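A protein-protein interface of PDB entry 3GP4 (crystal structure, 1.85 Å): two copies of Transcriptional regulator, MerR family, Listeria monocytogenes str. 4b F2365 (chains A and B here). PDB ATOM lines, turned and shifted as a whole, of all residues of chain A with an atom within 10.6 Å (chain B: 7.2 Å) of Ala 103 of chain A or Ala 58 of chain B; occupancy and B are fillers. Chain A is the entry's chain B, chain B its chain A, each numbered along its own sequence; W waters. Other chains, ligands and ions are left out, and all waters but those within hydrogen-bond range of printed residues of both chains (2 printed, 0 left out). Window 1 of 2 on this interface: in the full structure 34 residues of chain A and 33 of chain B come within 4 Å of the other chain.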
ATOM      1  N   ASN A  95     -23.983  15.665  12.493  1.00  0.00           N
ATOM      2  CA  ASN A  95     -24.340  16.891  13.240  1.00  0.00           C
ATOM      3  C   ASN A  95     -24.215  18.139  12.393  1.00  0.00           C
ATOM      4  O   ASN A  95     -25.130  19.001  12.454  1.00  0.00           O
ATOM      5  CB  ASN A  95     -23.562  17.041  14.530  1.00  0.00           C
ATOM      6  CG  ASN A  95     -24.003  16.041  15.584  1.00  0.00           C
ATOM      7  OD1 ASN A  95     -25.063  15.424  15.452  1.00  0.00           O
ATOM      8  ND2 ASN A  95     -23.180  15.850  16.618  1.00  0.00           N
ATOM      9  N   ARG A  96     -23.128  18.250  11.612  1.00  0.00           N
ATOM     10  CA  ARG A  96     -22.950  19.382  10.660  1.00  0.00           C
ATOM     11  C   ARG A  96     -24.030  19.425   9.586  1.00  0.00           C
ATOM     12  O   ARG A  96     -24.517  20.526   9.202  1.00  0.00           O
ATOM     13  CB  ARG A  96     -21.568  19.387   9.988  1.00  0.00           C
ATOM     14  CG  ARG A  96     -20.427  19.814  10.924  1.00  0.00           C
ATOM     15  CD  ARG A  96     -19.116  20.113  10.188  1.00  0.00           C
ATOM     16  NE  ARG A  96     -18.538  18.967   9.432  1.00  0.00           N
ATOM     17  CZ  ARG A  96     -17.839  17.955   9.972  1.00  0.00           C
ATOM     18  NH1 ARG A  96     -17.636  17.889  11.271  1.00  0.00           N
ATOM     19  NH2 ARG A  96     -17.345  16.990   9.205  1.00  0.00           N
ATOM     20  N   ILE A  97     -24.353  18.242   9.048  1.00  0.00           N
ATOM     21  CA  ILE A  97     -25.450  18.090   8.108  1.00  0.00           C
ATOM     22  C   ILE A  97     -26.765  18.575   8.739  1.00  0.00           C
ATOM     23  O   ILE A  97     -27.513  19.358   8.104  1.00  0.00           O
ATOM     24  CB  ILE A  97     -25.575  16.633   7.556  1.00  0.00           C
ATOM     25  CG1 ILE A  97     -24.330  16.278   6.716  1.00  0.00           C
ATOM     26  CG2 ILE A  97     -26.863  16.469   6.752  1.00  0.00           C
ATOM     27  CD1 ILE A  97     -24.325  14.897   5.998  1.00  0.00           C
ATOM     28  N   ASP A  98     -27.033  18.152   9.976  1.00  0.00           N
ATOM     29  CA  ASP A  98     -28.282  18.508  10.673  1.00  0.00           C
ATOM     30  C   ASP A  98     -28.411  20.016  10.866  1.00  0.00           C
ATOM     31  O   ASP A  98     -29.514  20.579  10.655  1.00  0.00           O
ATOM     32  CB  ASP A  98     -28.432  17.763  12.014  1.00  0.00           C
ATOM     33  CG  ASP A  98     -28.730  16.277  11.837  1.00  0.00           C
ATOM     34  OD1 ASP A  98     -29.053  15.856  10.701  1.00  0.00           O
ATOM     35  OD2 ASP A  98     -28.630  15.538  12.852  1.00  0.00           O
ATOM     36  N   VAL A  99     -27.287  20.659  11.203  1.00  0.00           N
ATOM     37  CA  VAL A  99     -27.204  22.098  11.355  1.00  0.00           C
ATOM     38  C   VAL A  99     -27.576  22.808  10.039  1.00  0.00           C
ATOM     39  O   VAL A  99     -28.472  23.678  10.020  1.00  0.00           O
ATOM     40  CB  VAL A  99     -25.836  22.543  11.932  1.00  0.00           C
ATOM     41  CG1 VAL A  99     -25.614  24.056  11.769  1.00  0.00           C
ATOM     42  CG2 VAL A  99     -25.713  22.144  13.449  1.00  0.00           C
ATOM     43  N   MET A 100     -26.910  22.409   8.954  1.00  0.00           N
ATOM     44  CA  MET A 100     -27.146  22.937   7.610  1.00  0.00           C
ATOM     45  C   MET A 100     -28.602  22.718   7.169  1.00  0.00           C
ATOM     46  O   MET A 100     -29.200  23.602   6.510  1.00  0.00           O
ATOM     47  CB  MET A 100     -26.143  22.328   6.580  1.00  0.00           C
ATOM     48  CG  MET A 100     -24.707  23.044   6.454  1.00  0.00           C
ATOM     49  SD  MET A 100     -23.454  21.843   5.736  1.00  0.00           S
ATOM     50  CE  MET A 100     -22.195  22.356   6.902  1.00  0.00           C
ATOM     51  N   GLN A 101     -29.170  21.557   7.500  1.00  0.00           N
ATOM     52  CA  GLN A 101     -30.552  21.266   7.110  1.00  0.00           C
ATOM     53  C   GLN A 101     -31.564  22.160   7.864  1.00  0.00           C
ATOM     54  O   GLN A 101     -32.563  22.592   7.295  1.00  0.00           O
ATOM     55  CB  GLN A 101     -30.887  19.774   7.305  1.00  0.00           C
ATOM     56  CG  GLN A 101     -32.298  19.395   6.841  1.00  0.00           C
ATOM     57  CD  GLN A 101     -32.456  19.443   5.329  1.00  0.00           C
ATOM     58  OE1 GLN A 101     -31.690  18.836   4.595  1.00  0.00           O
ATOM     59  NE2 GLN A 101     -33.448  20.206   4.851  1.00  0.00           N
ATOM     60  N   GLU A 102     -31.300  22.422   9.131  1.00  0.00           N
ATOM     61  CA  GLU A 102     -32.116  23.376   9.858  1.00  0.00           C
ATOM     62  C   GLU A 102     -32.108  24.758   9.207  1.00  0.00           C
ATOM     63  O   GLU A 102     -33.164  25.422   9.167  1.00  0.00           O
ATOM     64  CB  GLU A 102     -31.671  23.506  11.286  1.00  0.00           C
ATOM     65  CG  GLU A 102     -32.178  22.426  12.175  1.00  0.00           C
ATOM     66  CD  GLU A 102     -31.268  22.231  13.328  1.00  0.00           C
ATOM     67  OE1 GLU A 102     -30.848  23.260  13.928  1.00  0.00           O
ATOM     68  OE2 GLU A 102     -30.941  21.055  13.617  1.00  0.00           O
ATOM     69  N   ALA A 103     -30.952  25.209   8.728  1.00  0.00           N
ATOM     70  CA  ALA A 103     -30.864  26.483   7.968  1.00  0.00           C
ATOM     71  C   ALA A 103     -31.628  26.442   6.617  1.00  0.00           C
ATOM     72  O   ALA A 103     -32.281  27.459   6.191  1.00  0.00           O
ATOM     73  CB  ALA A 103     -29.380  26.954   7.754  1.00  0.00           C
ATOM     74  N   LEU A 104     -31.537  25.312   5.919  1.00  0.00           N
ATOM     75  CA  LEU A 104     -32.249  25.137   4.646  1.00  0.00           C
ATOM     76  C   LEU A 104     -33.755  25.185   4.924  1.00  0.00           C
ATOM     77  O   LEU A 104     -34.500  25.813   4.153  1.00  0.00           O
ATOM     78  CB  LEU A 104     -31.902  23.813   3.941  1.00  0.00           C
ATOM     79  CG  LEU A 104     -32.517  23.613   2.555  1.00  0.00           C
ATOM     80  CD1 LEU A 104     -31.922  24.650   1.541  1.00  0.00           C
ATOM     81  CD2 LEU A 104     -32.357  22.160   1.965  1.00  0.00           C
ATOM     82  N   ASP A 105     -34.192  24.513   5.996  1.00  0.00           N
ATOM     83  CA  ASP A 105     -35.608  24.558   6.421  1.00  0.00           C
ATOM     84  C   ASP A 105     -36.031  26.003   6.743  1.00  0.00           C
ATOM     85  O   ASP A 105     -37.156  26.444   6.379  1.00  0.00           O
ATOM     86  CB  ASP A 105     -35.855  23.666   7.644  1.00  0.00           C
ATOM     87  CG  ASP A 105     -35.686  22.169   7.345  1.00  0.00           C
ATOM     88  OD1 ASP A 105     -35.675  21.761   6.162  1.00  0.00           O
ATOM     89  OD2 ASP A 105     -35.547  21.424   8.330  1.00  0.00           O
ATOM     90  N   ARG A 106     -35.160  26.743   7.415  1.00  0.00           N
ATOM     91  CA  ARG A 106     -35.447  28.172   7.706  1.00  0.00           C
ATOM     92  C   ARG A 106     -35.569  29.008   6.430  1.00  0.00           C
ATOM     93  O   ARG A 106     -36.524  29.794   6.279  1.00  0.00           O
ATOM     94  CB  ARG A 106     -34.468  28.782   8.741  1.00  0.00           C
ATOM     95  CG  ARG A 106     -34.628  30.323   8.883  1.00  0.00           C
ATOM     96  CD  ARG A 106     -34.980  30.765  10.300  1.00  0.00           C
ATOM     97  NE  ARG A 106     -35.344  29.678  11.216  1.00  0.00           N
ATOM     98  CZ  ARG A 106     -35.288  29.776  12.548  1.00  0.00           C
ATOM     99  NH1 ARG A 106     -35.623  28.749  13.321  1.00  0.00           N
ATOM    100  NH2 ARG A 106     -34.875  30.899  13.114  1.00  0.00           N
ATOM    101  N   LEU A 107     -34.626  28.838   5.501  1.00  0.00           N
ATOM    102  CA  LEU A 107     -34.672  29.466   4.194  1.00  0.00           C
ATOM    103  C   LEU A 107     -35.945  29.122   3.407  1.00  0.00           C
ATOM    104  O   LEU A 107     -36.567  30.022   2.827  1.00  0.00           O
ATOM    105  CB  LEU A 107     -33.412  29.118   3.396  1.00  0.00           C
ATOM    106  CG  LEU A 107     -32.818  29.907   2.265  1.00  0.00           C
ATOM    107  CD1 LEU A 107     -32.872  31.427   2.553  1.00  0.00           C
ATOM    108  CD2 LEU A 107     -31.326  29.408   2.043  1.00  0.00           C
ATOM    109  N   ASP A 108     -36.349  27.846   3.429  1.00  0.00           N
ATOM    110  CA  ASP A 108     -37.589  27.394   2.788  1.00  0.00           C
ATOM    111  C   ASP A 108     -38.847  28.068   3.370  1.00  0.00           C
ATOM    112  O   ASP A 108     -39.771  28.410   2.616  1.00  0.00           O
ATOM    113  CB  ASP A 108     -37.768  25.877   2.908  1.00  0.00           C
ATOM    114  CG  ASP A 108     -36.929  25.085   1.900  1.00  0.00           C
ATOM    115  OD1 ASP A 108     -36.281  25.666   0.998  1.00  0.00           O
ATOM    116  OD2 ASP A 108     -36.889  23.840   2.055  1.00  0.00           O
ATOM    117  N   PHE A 109     -38.875  28.229   4.687  1.00  0.00           N
ATOM    118  CA  PHE A 109     -39.972  28.929   5.371  1.00  0.00           C
ATOM    119  C   PHE A 109     -40.042  30.394   4.912  1.00  0.00           C
ATOM    120  O   PHE A 109     -41.136  30.904   4.562  1.00  0.00           O
ATOM    121  CB  PHE A 109     -39.809  28.855   6.884  1.00  0.00           C
ATOM    122  CG  PHE A 109     -40.970  29.450   7.657  1.00  0.00           C
ATOM    123  CD1 PHE A 109     -42.137  28.703   7.867  1.00  0.00           C
ATOM    124  CD2 PHE A 109     -40.887  30.743   8.178  1.00  0.00           C
ATOM    125  CE1 PHE A 109     -43.219  29.246   8.591  1.00  0.00           C
ATOM    126  CE2 PHE A 109     -41.974  31.305   8.913  1.00  0.00           C
ATOM    127  CZ  PHE A 109     -43.131  30.554   9.118  1.00  0.00           C
ATOM    128  N   LYS A 110     -38.894  31.060   4.910  1.00  0.00           N
ATOM    129  CA  LYS A 110     -38.836  32.474   4.469  1.00  0.00           C
ATOM    130  C   LYS A 110     -39.280  32.593   3.014  1.00  0.00           C
ATOM    131  O   LYS A 110     -40.049  33.514   2.671  1.00  0.00           O
ATOM    132  CB  LYS A 110     -37.440  33.096   4.619  1.00  0.00           C
ATOM    133  CG  LYS A 110     -36.798  33.125   6.040  1.00  0.00           C
ATOM    134  CD  LYS A 110     -37.725  33.534   7.209  1.00  0.00           C
ATOM    135  CE  LYS A 110     -36.943  34.297   8.322  1.00  0.00           C
ATOM    136  NZ  LYS A 110     -37.091  33.711   9.704  1.00  0.00           N
ATOM    137  N   ILE A 111     -38.815  31.684   2.154  1.00  0.00           N
ATOM    138  CA  ILE A 111     -39.152  31.705   0.735  1.00  0.00           C
ATOM    139  C   ILE A 111     -40.647  31.466   0.492  1.00  0.00           C
ATOM    140  O   ILE A 111     -41.267  32.187  -0.285  1.00  0.00           O
ATOM    141  CB  ILE A 111     -38.291  30.698  -0.113  1.00  0.00           C
ATOM    142  CG1 ILE A 111     -36.883  31.231  -0.295  1.00  0.00           C
ATOM    143  CG2 ILE A 111     -38.873  30.507  -1.505  1.00  0.00           C
ATOM    144  CD1 ILE A 111     -35.800  30.096  -0.653  1.00  0.00           C
ATOM    145  N   PHE B  51     -30.827  35.282  12.530  1.00  0.00           N
ATOM    146  CA  PHE B  51     -30.827  34.884  11.114  1.00  0.00           C
ATOM    147  C   PHE B  51     -29.423  34.938  10.491  1.00  0.00           C
ATOM    148  O   PHE B  51     -29.024  33.979   9.773  1.00  0.00           O
ATOM    149  CB  PHE B  51     -31.834  35.731  10.333  1.00  0.00           C
ATOM    150  CG  PHE B  51     -31.953  35.385   8.867  1.00  0.00           C
ATOM    151  CD1 PHE B  51     -32.637  34.243   8.450  1.00  0.00           C
ATOM    152  CD2 PHE B  51     -31.418  36.231   7.921  1.00  0.00           C
ATOM    153  CE1 PHE B  51     -32.760  33.959   7.082  1.00  0.00           C
ATOM    154  CE2 PHE B  51     -31.542  35.947   6.537  1.00  0.00           C
ATOM    155  CZ  PHE B  51     -32.209  34.829   6.135  1.00  0.00           C
ATOM    156  N   THR B  52     -28.679  36.024  10.764  1.00  0.00           N
ATOM    157  CA  THR B  52     -27.338  36.223  10.193  1.00  0.00           C
ATOM    158  C   THR B  52     -26.395  35.132  10.652  1.00  0.00           C
ATOM    159  O   THR B  52     -25.754  34.453   9.811  1.00  0.00           O
ATOM    160  CB  THR B  52     -26.742  37.604  10.567  1.00  0.00           C
ATOM    161  OG1 THR B  52     -27.577  38.618  10.024  1.00  0.00           O
ATOM    162  CG2 THR B  52     -25.307  37.793   9.984  1.00  0.00           C
ATOM    163  N   ARG B  53     -26.352  34.935  11.969  1.00  0.00           N
ATOM    164  CA  ARG B  53     -25.546  33.886  12.575  1.00  0.00           C
ATOM    165  C   ARG B  53     -25.845  32.519  11.928  1.00  0.00           C
ATOM    166  O   ARG B  53     -24.917  31.829  11.492  1.00  0.00           O
ATOM    167  CB  ARG B  53     -25.736  33.825  14.094  1.00  0.00           C
ATOM    168  CG  ARG B  53     -24.756  32.844  14.794  1.00  0.00           C
ATOM    169  CD  ARG B  53     -23.298  33.271  14.507  1.00  0.00           C
ATOM    170  NE  ARG B  53     -22.314  32.186  14.649  1.00  0.00           N
ATOM    171  CZ  ARG B  53     -21.571  31.715  13.649  1.00  0.00           C
ATOM    172  NH1 ARG B  53     -21.683  32.230  12.423  1.00  0.00           N
ATOM    173  NH2 ARG B  53     -20.708  30.728  13.876  1.00  0.00           N
ATOM    174  N   GLN B  54     -27.121  32.172  11.814  1.00  0.00           N
ATOM    175  CA  GLN B  54     -27.519  30.831  11.321  1.00  0.00           C
ATOM    176  C   GLN B  54     -27.140  30.667   9.872  1.00  0.00           C
ATOM    177  O   GLN B  54     -26.581  29.611   9.455  1.00  0.00           O
ATOM    178  CB  GLN B  54     -29.006  30.584  11.549  1.00  0.00           C
ATOM    179  CG  GLN B  54     -29.506  29.182  11.097  1.00  0.00           C
ATOM    180  CD  GLN B  54     -31.031  28.972  11.152  1.00  0.00           C
ATOM    181  OE1 GLN B  54     -31.824  29.927  11.119  1.00  0.00           O
ATOM    182  NE2 GLN B  54     -31.445  27.698  11.218  1.00  0.00           N
ATOM    183  N   MET B  55     -27.415  31.712   9.083  1.00  0.00           N
ATOM    184  CA  MET B  55     -27.057  31.699   7.666  1.00  0.00           C
ATOM    185  C   MET B  55     -25.560  31.669   7.406  1.00  0.00           C
ATOM    186  O   MET B  55     -25.113  30.916   6.553  1.00  0.00           O
ATOM    187  CB  MET B  55     -27.730  32.844   6.882  1.00  0.00           C
ATOM    188  CG  MET B  55     -29.265  32.652   6.742  1.00  0.00           C
ATOM    189  SD  MET B  55     -29.880  31.047   6.115  1.00  0.00           S
ATOM    190  CE  MET B  55     -31.045  30.660   7.379  1.00  0.00           C
ATOM    191  N   ARG B  56     -24.786  32.461   8.147  1.00  0.00           N
ATOM    192  CA  ARG B  56     -23.338  32.446   7.985  1.00  0.00           C
ATOM    193  C   ARG B  56     -22.744  31.080   8.329  1.00  0.00           C
ATOM    194  O   ARG B  56     -21.816  30.626   7.656  1.00  0.00           O
ATOM    195  CB  ARG B  56     -22.679  33.539   8.837  1.00  0.00           C
ATOM    196  CG  ARG B  56     -22.835  34.932   8.214  1.00  0.00           C
ATOM    197  CD  ARG B  56     -22.083  35.083   6.899  1.00  0.00           C
ATOM    198  NE  ARG B  56     -20.638  34.961   7.114  1.00  0.00           N
ATOM    199  CZ  ARG B  56     -19.810  34.200   6.404  1.00  0.00           C
ATOM    200  NH1 ARG B  56     -20.236  33.467   5.385  1.00  0.00           N
ATOM    201  NH2 ARG B  56     -18.526  34.182   6.725  1.00  0.00           N
ATOM    202  N   ARG B  57     -23.252  30.486   9.408  1.00  0.00           N
ATOM    203  CA  ARG B  57     -22.820  29.173   9.877  1.00  0.00           C
ATOM    204  C   ARG B  57     -23.115  28.134   8.801  1.00  0.00           C
ATOM    205  O   ARG B  57     -22.324  27.230   8.601  1.00  0.00           O
ATOM    206  CB  ARG B  57     -23.528  28.853  11.187  1.00  0.00           C
ATOM    207  CG  ARG B  57     -23.216  27.539  11.851  1.00  0.00           C
ATOM    208  CD  ARG B  57     -23.568  27.699  13.338  1.00  0.00           C
ATOM    209  NE  ARG B  57     -23.250  26.499  14.096  1.00  0.00           N
ATOM    210  CZ  ARG B  57     -24.097  25.830  14.881  1.00  0.00           C
ATOM    211  NH1 ARG B  57     -25.350  26.251  15.069  1.00  0.00           N
ATOM    212  NH2 ARG B  57     -23.673  24.731  15.497  1.00  0.00           N
ATOM    213  N   ALA B  58     -24.225  28.295   8.073  1.00  0.00           N
ATOM    214  CA  ALA B  58     -24.546  27.426   6.921  1.00  0.00           C
ATOM    215  C   ALA B  58     -23.809  27.742   5.606  1.00  0.00           C
ATOM    216  O   ALA B  58     -24.069  27.088   4.590  1.00  0.00           O
ATOM    217  CB  ALA B  58     -26.053  27.389   6.679  1.00  0.00           C
ATOM    218  N   GLY B  59     -22.967  28.782   5.622  1.00  0.00           N
ATOM    219  CA  GLY B  59     -22.082  29.155   4.502  1.00  0.00           C
ATOM    220  C   GLY B  59     -22.673  30.098   3.471  1.00  0.00           C
ATOM    221  O   GLY B  59     -22.135  30.241   2.378  1.00  0.00           O
ATOM    222  N   LEU B  60     -23.804  30.734   3.781  1.00  0.00           N
ATOM    223  CA  LEU B  60     -24.313  31.755   2.847  1.00  0.00           C
ATOM    224  C   LEU B  60     -23.279  32.855   2.806  1.00  0.00           C
ATOM    225  O   LEU B  60     -22.746  33.262   3.855  1.00  0.00           O
ATOM    226  CB  LEU B  60     -25.670  32.328   3.295  1.00  0.00           C
ATOM    227  CG  LEU B  60     -26.882  31.497   2.839  1.00  0.00           C
ATOM    228  CD1 LEU B  60     -26.979  30.173   3.599  1.00  0.00           C
ATOM    229  CD2 LEU B  60     -28.205  32.300   2.991  1.00  0.00           C
ATOM    230  N   SER B  61     -22.992  33.356   1.608  1.00  0.00           N
ATOM    231  CA  SER B  61     -21.954  34.373   1.493  1.00  0.00           C
ATOM    232  C   SER B  61     -22.346  35.674   2.168  1.00  0.00           C
ATOM    233  O   SER B  61     -23.533  36.060   2.186  1.00  0.00           O
ATOM    234  CB  SER B  61     -21.506  34.598   0.037  1.00  0.00           C
ATOM    235  OG  SER B  61     -22.179  35.675  -0.620  1.00  0.00           O
ATOM    236  N   ARG B  90     -30.673  29.154  -1.634  1.00  0.00           N
ATOM    237  CA  ARG B  90     -31.292  27.859  -1.313  1.00  0.00           C
ATOM    238  C   ARG B  90     -30.727  26.724  -2.154  1.00  0.00           C
ATOM    239  O   ARG B  90     -30.311  25.665  -1.604  1.00  0.00           O
ATOM    240  CB  ARG B  90     -32.827  27.959  -1.461  1.00  0.00           C
ATOM    241  CG  ARG B  90     -33.649  26.889  -0.713  1.00  0.00           C
ATOM    242  CD  ARG B  90     -33.669  25.482  -1.396  1.00  0.00           C
ATOM    243  NE  ARG B  90     -34.542  24.596  -0.620  1.00  0.00           N
ATOM    244  CZ  ARG B  90     -34.640  23.266  -0.715  1.00  0.00           C
ATOM    245  NH1 ARG B  90     -35.447  22.606   0.131  1.00  0.00           N
ATOM    246  NH2 ARG B  90     -33.935  22.595  -1.601  1.00  0.00           N
ATOM    247  N   GLU B  92     -27.872  26.630  -3.744  1.00  0.00           N
ATOM    248  CA  GLU B  92     -26.451  26.438  -3.430  1.00  0.00           C
ATOM    249  C   GLU B  92     -26.258  25.735  -2.097  1.00  0.00           C
ATOM    250  O   GLU B  92     -25.327  24.906  -1.953  1.00  0.00           O
ATOM    251  CB  GLU B  92     -25.693  27.763  -3.480  1.00  0.00           C
ATOM    252  CG  GLU B  92     -25.690  28.346  -4.911  1.00  0.00           C
ATOM    253  CD  GLU B  92     -25.068  29.720  -5.035  1.00  0.00           C
ATOM    254  OE1 GLU B  92     -24.307  30.144  -4.141  1.00  0.00           O
ATOM    255  OE2 GLU B  92     -25.329  30.381  -6.065  1.00  0.00           O
ATOM    256  N   LEU B  93     -27.096  26.071  -1.117  1.00  0.00           N
ATOM    257  CA  LEU B  93     -27.047  25.397   0.181  1.00  0.00           C
ATOM    258  C   LEU B  93     -27.475  23.930   0.015  1.00  0.00           C
ATOM    259  O   LEU B  93     -26.847  23.030   0.605  1.00  0.00           O
ATOM    260  CB  LEU B  93     -27.927  26.103   1.252  1.00  0.00           C
ATOM    261  CG  LEU B  93     -28.063  25.404   2.637  1.00  0.00           C
ATOM    262  CD1 LEU B  93     -26.699  25.067   3.333  1.00  0.00           C
ATOM    263  CD2 LEU B  93     -28.931  26.227   3.594  1.00  0.00           C
ATOM    264  N   ARG B  96     -24.605  22.011  -1.378  1.00  0.00           N
ATOM    265  CA  ARG B  96     -23.613  21.757  -0.300  1.00  0.00           C
ATOM    266  C   ARG B  96     -23.995  20.603   0.621  1.00  0.00           C
ATOM    267  O   ARG B  96     -23.148  19.713   0.928  1.00  0.00           O
ATOM    268  CB  ARG B  96     -23.311  23.017   0.522  1.00  0.00           C
ATOM    269  CG  ARG B  96     -22.463  24.068  -0.205  1.00  0.00           C
ATOM    270  CD  ARG B  96     -21.923  25.153   0.758  1.00  0.00           C
ATOM    271  NE  ARG B  96     -22.969  25.922   1.466  1.00  0.00           N
ATOM    272  CZ  ARG B  96     -23.651  26.943   0.931  1.00  0.00           C
ATOM    273  NH1 ARG B  96     -23.446  27.303  -0.322  1.00  0.00           N
ATOM    274  NH2 ARG B  96     -24.558  27.594   1.652  1.00  0.00           N
ATOM    275  N   ILE B  97     -25.258  20.598   1.051  1.00  0.00           N
ATOM    276  CA  ILE B  97     -25.792  19.499   1.871  1.00  0.00           C
ATOM    277  C   ILE B  97     -25.698  18.161   1.123  1.00  0.00           C
ATOM    278  O   ILE B  97     -25.240  17.133   1.696  1.00  0.00           O
ATOM    279  CB  ILE B  97     -27.235  19.773   2.358  1.00  0.00           C
ATOM    280  CG1 ILE B  97     -27.220  20.878   3.422  1.00  0.00           C
ATOM    281  CG2 ILE B  97     -27.922  18.500   2.909  1.00  0.00           C
ATOM    282  CD1 ILE B  97     -28.611  21.506   3.679  1.00  0.00           C
HETATM  283  O   HOH W   1     -21.979  24.944   4.149  1.00  0.00           O
HETATM  284  O   HOH W   2     -28.960  25.858  11.361  1.00  0.00           O
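Positions printed for both chains: 96 and 97. Of the 15 pairs that touch across the chains among the printed residues, none has its exchanged pair printed and touching as well.
Ala 103 of chain A touches just these residues of chain B: Gln 54, Met 55 and Ala 58. Asp 105 of chain A touches none of the printed residues of chain B. Of the printed residues of chain B, Ile 111 of chain A touches Arg 90 (3.7 Å). Of chain A, only Glu 102 (3.5 Å), Ala 103 (3.5 Å) and Arg 106 (3.4 Å) come within 4 Å of Gln 54 of chain B. Printed residues of chain A within 4 Å of Met 55 of chain B: Ala 103 and Arg 106. Ala 58 of chain B touches just one residue of chain A: Ala 103 (3.5 Å). No residue of chain A comes within 4 Å of Gly 59 of chain B. Ser 61 of chain B touches none of the printed residues of chain A. Printed residues of chain A within 4 Å of Arg 90 of chain B: Leu 104 (3.4 Å), Leu 107 (3.7 Å), Asp 108 (2.6 Å) and Ile 111 (3.7 Å). Leu 93 of chain B touches two residues of chain A.
The side-chain carboxylate (OD1) of Asp 108 of chain A is in salt-bridge range of the guanidinium group (NE) of Arg 90 of chain B, at 2.6 Å.
Among the printed residues, pairs that only touch across the chains: Arg 106 of chain A with Gln 54 of chain B (3.4 Å), Leu 104 of chain A with Arg 90 of chain B (3.4 Å), Glu 102 of chain A with Gln 54 of chain B (3.5 Å), Ala 103 of chain A with Gln 54 of chain B (3.5 Å), Ala 103 of chain A with Ala 58 of chain B (3.5 Å), Met 100 of chain A with Ile 97 of chain B (3.6 Å), Leu 104 of chain A with Leu 93 of chain B (3.6 Å), Ala 103 of chain A with Met 55 of chain B (3.6 Å), Leu 107 of chain A with Arg 90 of chain B (3.7 Å), Ile 111 of chain A with Arg 90 of chain B (3.7 Å), Gln 101 of chain A with Ile 97 of chain B (3.9 Å), Val 99 of chain A with Arg 57 of chain B (3.9 Å), Arg 106 of chain A with Met 55 of chain B (3.9 Å) and Met 100 of chain A with Leu 93 of chain B (3.9 Å).
The backbone carbonyl oxygen (O) of Met 55 of chain B is in hydrogen-bond range of the backbone NH (N) of Leu 60 of chain B (3.1 Å). The backbone carbonyl oxygen of Ala 58 of chain B lies within hydrogen-bond range of the guanidinium group of Arg 96 of chain B, at 3.0 Å. The side-chain amide nitrogen (NE2) of Gln 101 of chain A sits at hydrogen-bond distance from the side-chain carboxylate (OD1) of Asp 105 of chain A (3.0 Å).
Water W2 lies within hydrogen-bond range of O of Val 99 of chain A (2.6 Å), NE2 of Gln 54 of chain B (3.1 Å) and N of Ala 103 of chain A (3.4 Å). Water W1 lies within hydrogen-bond range of NE of Arg 96 of chain B, O of Ala 58 of chain B and SD of Met 100 of chain A.
Of the 16 printed residues of chain B, 7 touch a printed residue of chain A. Printed residues of chain B that touch a printed residue of chain A: Gln 54, Met 55, Arg 57, Ala 58, Arg 90, Leu 93 and Ile 97. Along chain B the printed residues that touch a printed residue of chain A span positions 54 to 97. Hydrophobic or aromatic side chains of chain A that line the printed part of chain B: Val 99, Met 100, Ala 103, Leu 104, Leu 107 and Ile 111.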
